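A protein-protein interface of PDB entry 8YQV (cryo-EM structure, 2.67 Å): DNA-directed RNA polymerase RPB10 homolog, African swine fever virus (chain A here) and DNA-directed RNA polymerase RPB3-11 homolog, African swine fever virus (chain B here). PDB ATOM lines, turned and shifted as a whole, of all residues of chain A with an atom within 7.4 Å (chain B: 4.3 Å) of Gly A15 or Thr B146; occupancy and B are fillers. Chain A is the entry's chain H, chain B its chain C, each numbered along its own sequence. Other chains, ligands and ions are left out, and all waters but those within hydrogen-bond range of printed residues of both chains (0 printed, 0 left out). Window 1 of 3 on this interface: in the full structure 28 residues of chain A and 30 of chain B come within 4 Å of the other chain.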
ATOM      1  N   ILE A   3      18.097 -24.981 -16.993  1.00  0.00           N
ATOM      2  CA  ILE A   3      18.124 -24.860 -15.532  1.00  0.00           C
ATOM      3  C   ILE A   3      18.229 -26.258 -14.933  1.00  0.00           C
ATOM      4  O   ILE A   3      17.456 -27.148 -15.322  1.00  0.00           O
ATOM      5  CB  ILE A   3      16.878 -24.130 -15.027  1.00  0.00           C
ATOM      6  CG1 ILE A   3      16.872 -22.687 -15.518  1.00  0.00           C
ATOM      7  CG2 ILE A   3      16.818 -24.147 -13.517  1.00  0.00           C
ATOM      8  CD1 ILE A   3      15.604 -21.944 -15.206  1.00  0.00           C
ATOM      9  N   PRO A   4      19.156 -26.507 -14.015  1.00  0.00           N
ATOM     10  CA  PRO A   4      19.384 -27.874 -13.545  1.00  0.00           C
ATOM     11  C   PRO A   4      18.169 -28.442 -12.830  1.00  0.00           C
ATOM     12  O   PRO A   4      17.293 -27.729 -12.349  1.00  0.00           O
ATOM     13  CB  PRO A   4      20.577 -27.721 -12.602  1.00  0.00           C
ATOM     14  CG  PRO A   4      20.550 -26.314 -12.194  1.00  0.00           C
ATOM     15  CD  PRO A   4      20.083 -25.561 -13.380  1.00  0.00           C
ATOM     16  N   VAL A   5      18.117 -29.771 -12.802  1.00  0.00           N
ATOM     17  CA  VAL A   5      17.007 -30.464 -12.160  1.00  0.00           C
ATOM     18  C   VAL A   5      16.974 -30.147 -10.673  1.00  0.00           C
ATOM     19  O   VAL A   5      15.910 -29.925 -10.090  1.00  0.00           O
ATOM     20  CB  VAL A   5      17.109 -31.977 -12.410  1.00  0.00           C
ATOM     21  CG1 VAL A   5      16.014 -32.701 -11.682  1.00  0.00           C
ATOM     22  CG2 VAL A   5      17.025 -32.262 -13.868  1.00  0.00           C
ATOM     23  N   VAL A   6      18.140 -30.129 -10.040  1.00  0.00           N
ATOM     24  CA  VAL A   6      18.270 -29.817  -8.629  1.00  0.00           C
ATOM     25  C   VAL A   6      19.284 -28.696  -8.491  1.00  0.00           C
ATOM     26  O   VAL A   6      20.096 -28.449  -9.381  1.00  0.00           O
ATOM     27  CB  VAL A   6      18.696 -31.044  -7.800  1.00  0.00           C
ATOM     28  CG1 VAL A   6      17.621 -32.104  -7.838  1.00  0.00           C
ATOM     29  CG2 VAL A   6      20.006 -31.591  -8.307  1.00  0.00           C
ATOM     30  N   CYS A   7      19.216 -27.997  -7.365  1.00  0.00           N
ATOM     31  CA  CYS A   7      20.214 -26.988  -7.064  1.00  0.00           C
ATOM     32  C   CYS A   7      21.590 -27.633  -6.977  1.00  0.00           C
ATOM     33  O   CYS A   7      21.759 -28.668  -6.334  1.00  0.00           O
ATOM     34  CB  CYS A   7      19.860 -26.287  -5.758  1.00  0.00           C
ATOM     35  SG  CYS A   7      21.104 -25.171  -5.118  1.00  0.00           S
ATOM     36  N   PHE A  12      18.014 -29.161  -3.653  1.00  0.00           N
ATOM     37  CA  PHE A  12      16.581 -28.934  -3.685  1.00  0.00           C
ATOM     38  C   PHE A  12      16.071 -29.041  -5.121  1.00  0.00           C
ATOM     39  O   PHE A  12      16.735 -28.574  -6.048  1.00  0.00           O
ATOM     40  CB  PHE A  12      16.260 -27.559  -3.104  1.00  0.00           C
ATOM     41  CG  PHE A  12      14.800 -27.271  -2.992  1.00  0.00           C
ATOM     42  CD1 PHE A  12      14.074 -27.724  -1.914  1.00  0.00           C
ATOM     43  CD2 PHE A  12      14.154 -26.537  -3.963  1.00  0.00           C
ATOM     44  CE1 PHE A  12      12.736 -27.458  -1.817  1.00  0.00           C
ATOM     45  CE2 PHE A  12      12.818 -26.273  -3.870  1.00  0.00           C
ATOM     46  CZ  PHE A  12      12.109 -26.731  -2.798  1.00  0.00           C
ATOM     47  N   PRO A  13      14.901 -29.644  -5.340  1.00  0.00           N
ATOM     48  CA  PRO A  13      14.415 -29.822  -6.711  1.00  0.00           C
ATOM     49  C   PRO A  13      14.029 -28.513  -7.374  1.00  0.00           C
ATOM     50  O   PRO A  13      12.852 -28.176  -7.485  1.00  0.00           O
ATOM     51  CB  PRO A  13      13.201 -30.736  -6.530  1.00  0.00           C
ATOM     52  CG  PRO A  13      12.768 -30.510  -5.150  1.00  0.00           C
ATOM     53  CD  PRO A  13      14.013 -30.294  -4.368  1.00  0.00           C
ATOM     54  N   ILE A  14      14.937 -27.711  -7.864  1.00  0.00           N
ATOM     55  CA  ILE A  14      14.569 -26.450  -8.464  1.00  0.00           C
ATOM     56  C   ILE A  14      14.062 -26.700  -9.860  1.00  0.00           C
ATOM     57  O   ILE A  14      13.419 -25.858 -10.404  1.00  0.00           O
ATOM     58  CB  ILE A  14      15.707 -25.400  -8.508  1.00  0.00           C
ATOM     59  CG1 ILE A  14      16.982 -25.967  -9.094  1.00  0.00           C
ATOM     60  CG2 ILE A  14      15.951 -24.829  -7.129  1.00  0.00           C
ATOM     61  CD1 ILE A  14      17.859 -24.895  -9.679  1.00  0.00           C
ATOM     62  N   GLY A  15      14.354 -27.846 -10.460  1.00  0.00           N
ATOM     63  CA  GLY A  15      13.918 -28.040 -11.829  1.00  0.00           C
ATOM     64  C   GLY A  15      12.430 -28.207 -12.019  1.00  0.00           C
ATOM     65  O   GLY A  15      11.904 -27.861 -13.079  1.00  0.00           O
ATOM     66  N   THR A  16      11.726 -28.729 -11.017  1.00  0.00           N
ATOM     67  CA  THR A  16      10.295 -28.945 -11.182  1.00  0.00           C
ATOM     68  C   THR A  16       9.521 -27.653 -11.367  1.00  0.00           C
ATOM     69  O   THR A  16       8.371 -27.699 -11.811  1.00  0.00           O
ATOM     70  CB  THR A  16       9.724 -29.724  -9.996  1.00  0.00           C
ATOM     71  OG1 THR A  16       8.297 -29.632 -10.007  1.00  0.00           O
ATOM     72  CG2 THR A  16      10.243 -29.198  -8.706  1.00  0.00           C
ATOM     73  N   TYR A  17      10.119 -26.511 -11.046  1.00  0.00           N
ATOM     74  CA  TYR A  17       9.516 -25.209 -11.272  1.00  0.00           C
ATOM     75  C   TYR A  17      10.244 -24.418 -12.343  1.00  0.00           C
ATOM     76  O   TYR A  17       9.867 -23.277 -12.613  1.00  0.00           O
ATOM     77  CB  TYR A  17       9.498 -24.407  -9.973  1.00  0.00           C
ATOM     78  CG  TYR A  17       8.967 -25.170  -8.796  1.00  0.00           C
ATOM     79  CD1 TYR A  17       7.620 -25.440  -8.676  1.00  0.00           C
ATOM     80  CD2 TYR A  17       9.818 -25.629  -7.808  1.00  0.00           C
ATOM     81  CE1 TYR A  17       7.133 -26.135  -7.605  1.00  0.00           C
ATOM     82  CE2 TYR A  17       9.340 -26.329  -6.733  1.00  0.00           C
ATOM     83  CZ  TYR A  17       7.996 -26.577  -6.635  1.00  0.00           C
ATOM     84  OH  TYR A  17       7.503 -27.274  -5.562  1.00  0.00           O
ATOM     85  N   ALA A  18      11.282 -24.991 -12.952  1.00  0.00           N
ATOM     86  CA  ALA A  18      12.107 -24.223 -13.878  1.00  0.00           C
ATOM     87  C   ALA A  18      11.303 -23.761 -15.081  1.00  0.00           C
ATOM     88  O   ALA A  18      11.266 -22.564 -15.386  1.00  0.00           O
ATOM     89  CB  ALA A  18      13.306 -25.052 -14.325  1.00  0.00           C
ATOM     90  N   ALA A  19      10.618 -24.689 -15.750  1.00  0.00           N
ATOM     91  CA  ALA A  19       9.880 -24.339 -16.958  1.00  0.00           C
ATOM     92  C   ALA A  19       8.902 -23.209 -16.688  1.00  0.00           C
ATOM     93  O   ALA A  19       8.968 -22.153 -17.330  1.00  0.00           O
ATOM     94  CB  ALA A  19       9.144 -25.563 -17.495  1.00  0.00           C
ATOM     95  N   ILE A  20       8.042 -23.380 -15.683  1.00  0.00           N
ATOM     96  CA  ILE A  20       7.112 -22.320 -15.317  1.00  0.00           C
ATOM     97  C   ILE A  20       7.874 -21.037 -15.036  1.00  0.00           C
ATOM     98  O   ILE A  20       7.575 -19.982 -15.606  1.00  0.00           O
ATOM     99  CB  ILE A  20       6.262 -22.742 -14.107  1.00  0.00           C
ATOM    100  CG1 ILE A  20       5.431 -23.978 -14.435  1.00  0.00           C
ATOM    101  CG2 ILE A  20       5.365 -21.608 -13.678  1.00  0.00           C
ATOM    102  CD1 ILE A  20       4.847 -24.649 -13.221  1.00  0.00           C
ATOM    103  N   ILE A  60       9.513 -21.869  -3.770  1.00  0.00           N
ATOM    104  CA  ILE A  60      10.935 -22.121  -3.568  1.00  0.00           C
ATOM    105  C   ILE A  60      11.383 -21.379  -2.316  1.00  0.00           C
ATOM    106  O   ILE A  60      10.959 -20.237  -2.096  1.00  0.00           O
ATOM    107  CB  ILE A  60      11.735 -21.707  -4.810  1.00  0.00           C
ATOM    108  CG1 ILE A  60      11.436 -22.673  -5.952  1.00  0.00           C
ATOM    109  CG2 ILE A  60      13.222 -21.650  -4.528  1.00  0.00           C
ATOM    110  CD1 ILE A  60      11.998 -22.243  -7.262  1.00  0.00           C
ATOM    111  N   LEU A  70      18.637 -20.697 -10.021  1.00  0.00           N
ATOM    112  CA  LEU A  70      17.413 -20.549 -10.790  1.00  0.00           C
ATOM    113  C   LEU A  70      17.437 -19.280 -11.631  1.00  0.00           C
ATOM    114  O   LEU A  70      16.976 -19.277 -12.775  1.00  0.00           O
ATOM    115  CB  LEU A  70      16.220 -20.549  -9.841  1.00  0.00           C
ATOM    116  CG  LEU A  70      14.823 -20.514 -10.426  1.00  0.00           C
ATOM    117  CD1 LEU A  70      14.440 -21.870 -10.951  1.00  0.00           C
ATOM    118  CD2 LEU A  70      13.871 -20.061  -9.360  1.00  0.00           C
ATOM    119  N   PHE B  30       1.381 -26.762 -18.655  1.00  0.00           N
ATOM    120  CA  PHE B  30       1.041 -28.103 -18.218  1.00  0.00           C
ATOM    121  C   PHE B  30      -0.426 -28.287 -17.866  1.00  0.00           C
ATOM    122  O   PHE B  30      -0.783 -29.341 -17.330  1.00  0.00           O
ATOM    123  CB  PHE B  30       1.893 -28.500 -17.002  1.00  0.00           C
ATOM    124  CG  PHE B  30       3.365 -28.280 -17.190  1.00  0.00           C
ATOM    125  CD1 PHE B  30       4.094 -29.081 -18.046  1.00  0.00           C
ATOM    126  CD2 PHE B  30       4.020 -27.280 -16.504  1.00  0.00           C
ATOM    127  CE1 PHE B  30       5.438 -28.882 -18.217  1.00  0.00           C
ATOM    128  CE2 PHE B  30       5.365 -27.079 -16.676  1.00  0.00           C
ATOM    129  CZ  PHE B  30       6.074 -27.882 -17.531  1.00  0.00           C
ATOM    130  N   LEU B  36       1.096 -29.895  -7.485  1.00  0.00           N
ATOM    131  CA  LEU B  36       1.780 -31.020  -8.094  1.00  0.00           C
ATOM    132  C   LEU B  36       1.561 -32.279  -7.258  1.00  0.00           C
ATOM    133  O   LEU B  36       1.353 -32.195  -6.046  1.00  0.00           O
ATOM    134  CB  LEU B  36       3.269 -30.727  -8.222  1.00  0.00           C
ATOM    135  CG  LEU B  36       3.664 -29.684  -9.265  1.00  0.00           C
ATOM    136  CD1 LEU B  36       5.122 -29.329  -9.127  1.00  0.00           C
ATOM    137  CD2 LEU B  36       3.381 -30.193 -10.657  1.00  0.00           C
ATOM    138  N   ASN B 144       7.195 -35.821 -10.528  1.00  0.00           N
ATOM    139  CA  ASN B 144       6.427 -34.714 -11.074  1.00  0.00           C
ATOM    140  C   ASN B 144       6.601 -34.635 -12.589  1.00  0.00           C
ATOM    141  O   ASN B 144       7.681 -34.924 -13.106  1.00  0.00           O
ATOM    142  CB  ASN B 144       6.861 -33.403 -10.436  1.00  0.00           C
ATOM    143  CG  ASN B 144       6.249 -33.196  -9.086  1.00  0.00           C
ATOM    144  OD1 ASN B 144       5.061 -33.427  -8.897  1.00  0.00           O
ATOM    145  ND2 ASN B 144       7.053 -32.765  -8.132  1.00  0.00           N
ATOM    146  N   PRO B 145       5.567 -34.231 -13.316  1.00  0.00           N
ATOM    147  CA  PRO B 145       5.638 -34.251 -14.781  1.00  0.00           C
ATOM    148  C   PRO B 145       6.209 -32.984 -15.396  1.00  0.00           C
ATOM    149  O   PRO B 145       6.042 -32.752 -16.595  1.00  0.00           O
ATOM    150  CB  PRO B 145       4.173 -34.437 -15.177  1.00  0.00           C
ATOM    151  CG  PRO B 145       3.439 -33.721 -14.117  1.00  0.00           C
ATOM    152  CD  PRO B 145       4.211 -33.909 -12.844  1.00  0.00           C
ATOM    153  N   THR B 146       6.873 -32.150 -14.601  1.00  0.00           N
ATOM    154  CA  THR B 146       7.254 -30.817 -15.048  1.00  0.00           C
ATOM    155  C   THR B 146       8.754 -30.636 -15.228  1.00  0.00           C
ATOM    156  O   THR B 146       9.203 -29.508 -15.451  1.00  0.00           O
ATOM    157  CB  THR B 146       6.724 -29.770 -14.070  1.00  0.00           C
ATOM    158  OG1 THR B 146       7.271 -30.020 -12.773  1.00  0.00           O
ATOM    159  CG2 THR B 146       5.221 -29.839 -13.991  1.00  0.00           C
ATOM    160  N   PHE B 147       9.542 -31.700 -15.144  1.00  0.00           N
ATOM    161  CA  PHE B 147      10.983 -31.571 -15.292  1.00  0.00           C
ATOM    162  C   PHE B 147      11.360 -31.479 -16.762  1.00  0.00           C
ATOM    163  O   PHE B 147      10.953 -32.317 -17.567  1.00  0.00           O
ATOM    164  CB  PHE B 147      11.696 -32.758 -14.655  1.00  0.00           C
ATOM    165  CG  PHE B 147      11.649 -32.770 -13.163  1.00  0.00           C
ATOM    166  CD1 PHE B 147      12.599 -32.101 -12.426  1.00  0.00           C
ATOM    167  CD2 PHE B 147      10.667 -33.469 -12.496  1.00  0.00           C
ATOM    168  CE1 PHE B 147      12.568 -32.128 -11.062  1.00  0.00           C
ATOM    169  CE2 PHE B 147      10.632 -33.491 -11.133  1.00  0.00           C
ATOM    170  CZ  PHE B 147      11.583 -32.820 -10.416  1.00  0.00           C
ATOM    171  N   GLU B 148      12.149 -30.470 -17.110  1.00  0.00           N
ATOM    172  CA  GLU B 148      12.676 -30.338 -18.465  1.00  0.00           C
ATOM    173  C   GLU B 148      13.808 -31.335 -18.645  1.00  0.00           C
ATOM    174  O   GLU B 148      14.953 -31.059 -18.288  1.00  0.00           O
ATOM    175  CB  GLU B 148      13.169 -28.921 -18.720  1.00  0.00           C
ATOM    176  CG  GLU B 148      12.086 -27.881 -18.830  1.00  0.00           C
ATOM    177  CD  GLU B 148      12.644 -26.479 -18.856  1.00  0.00           C
ATOM    178  OE1 GLU B 148      13.793 -26.282 -18.413  1.00  0.00           O
ATOM    179  OE2 GLU B 148      11.937 -25.569 -19.332  1.00  0.00           O
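Gly A15 touches just these residues of chain B: Thr B146 and Phe B147.
Of chain A, only Gly A15 (3.95 Å) and Thr A16 (2.7 Å) come within 4 Å of Thr B146.
Of the printed residues of chain B, Val A5 touches Phe B147 (3.5 Å).
Of the printed residues of chain B, Ile A20 touches Phe B30 (3.8 Å).
Of the printed residues of chain A, Phe B147 touches Val A5, Gly A15 and Thr A16.
Val A6 touches none of the printed residues of chain B.
Pro A13 touches none of the printed residues of chain B.
The nearest residue of chain A that does not touch Thr B146 is Ala A19 (4.4 Å).
The nearest printed residue of chain A that does not touch Glu B148 is Ala A18 (4.3 Å).
The backbone carbonyl oxygen (O) of Pro A4 lies close to the backbone NH (N) of Gly A15.
The backbone carbonyl oxygen of Val A5 sits at hydrogen-bond distance from the backbone NH of Gly A15 (2.6 Å).
The backbone carbonyl oxygen (O) of Val A5 lies within hydrogen-bond range of the backbone NH (N) of Ile A14, at 3.3 Å.
CD1 of Phe B147 touches CG1 of Val A5, at 3.5 Å.
O of Thr B146 touches O of Gly A15 (3.95 Å).
C of Gly A15 touches CD1 of Phe B147, 3.9 Å away.
Leu B36 touches Thr A16 (CD1 to OG1, 3.3 Å).
Thr A16 touches Asn B144 (OG1 to ND2, 3.9 Å).
Phe B147 touches Thr A16.
Phe B30 touches Ala A19 (CZ to CB, 3.8 Å).
OE2 of Glu B148 touches CB of Ala A19 (3.3 Å).
CE2 of Phe B30 touches CG1 of Ile A20 (3.8 Å).
Of the 7 printed residues of chain B, 6 touch a printed residue of chain A.
Hydrophobic or aromatic side chains of chain B within 4 Å of the printed part of chain A: Phe B30, Leu B36 and Phe B147.
Printed residues of chain A that touch a printed residue of chain B: Val A5, Gly A15, Thr A16, Ala A19 and Ile A20.
The backbone carbonyl oxygen (O) of Thr A16 sits at hydrogen-bond distance from the side-chain hydroxyl (OG1) of Thr B146 (2.7 Å).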
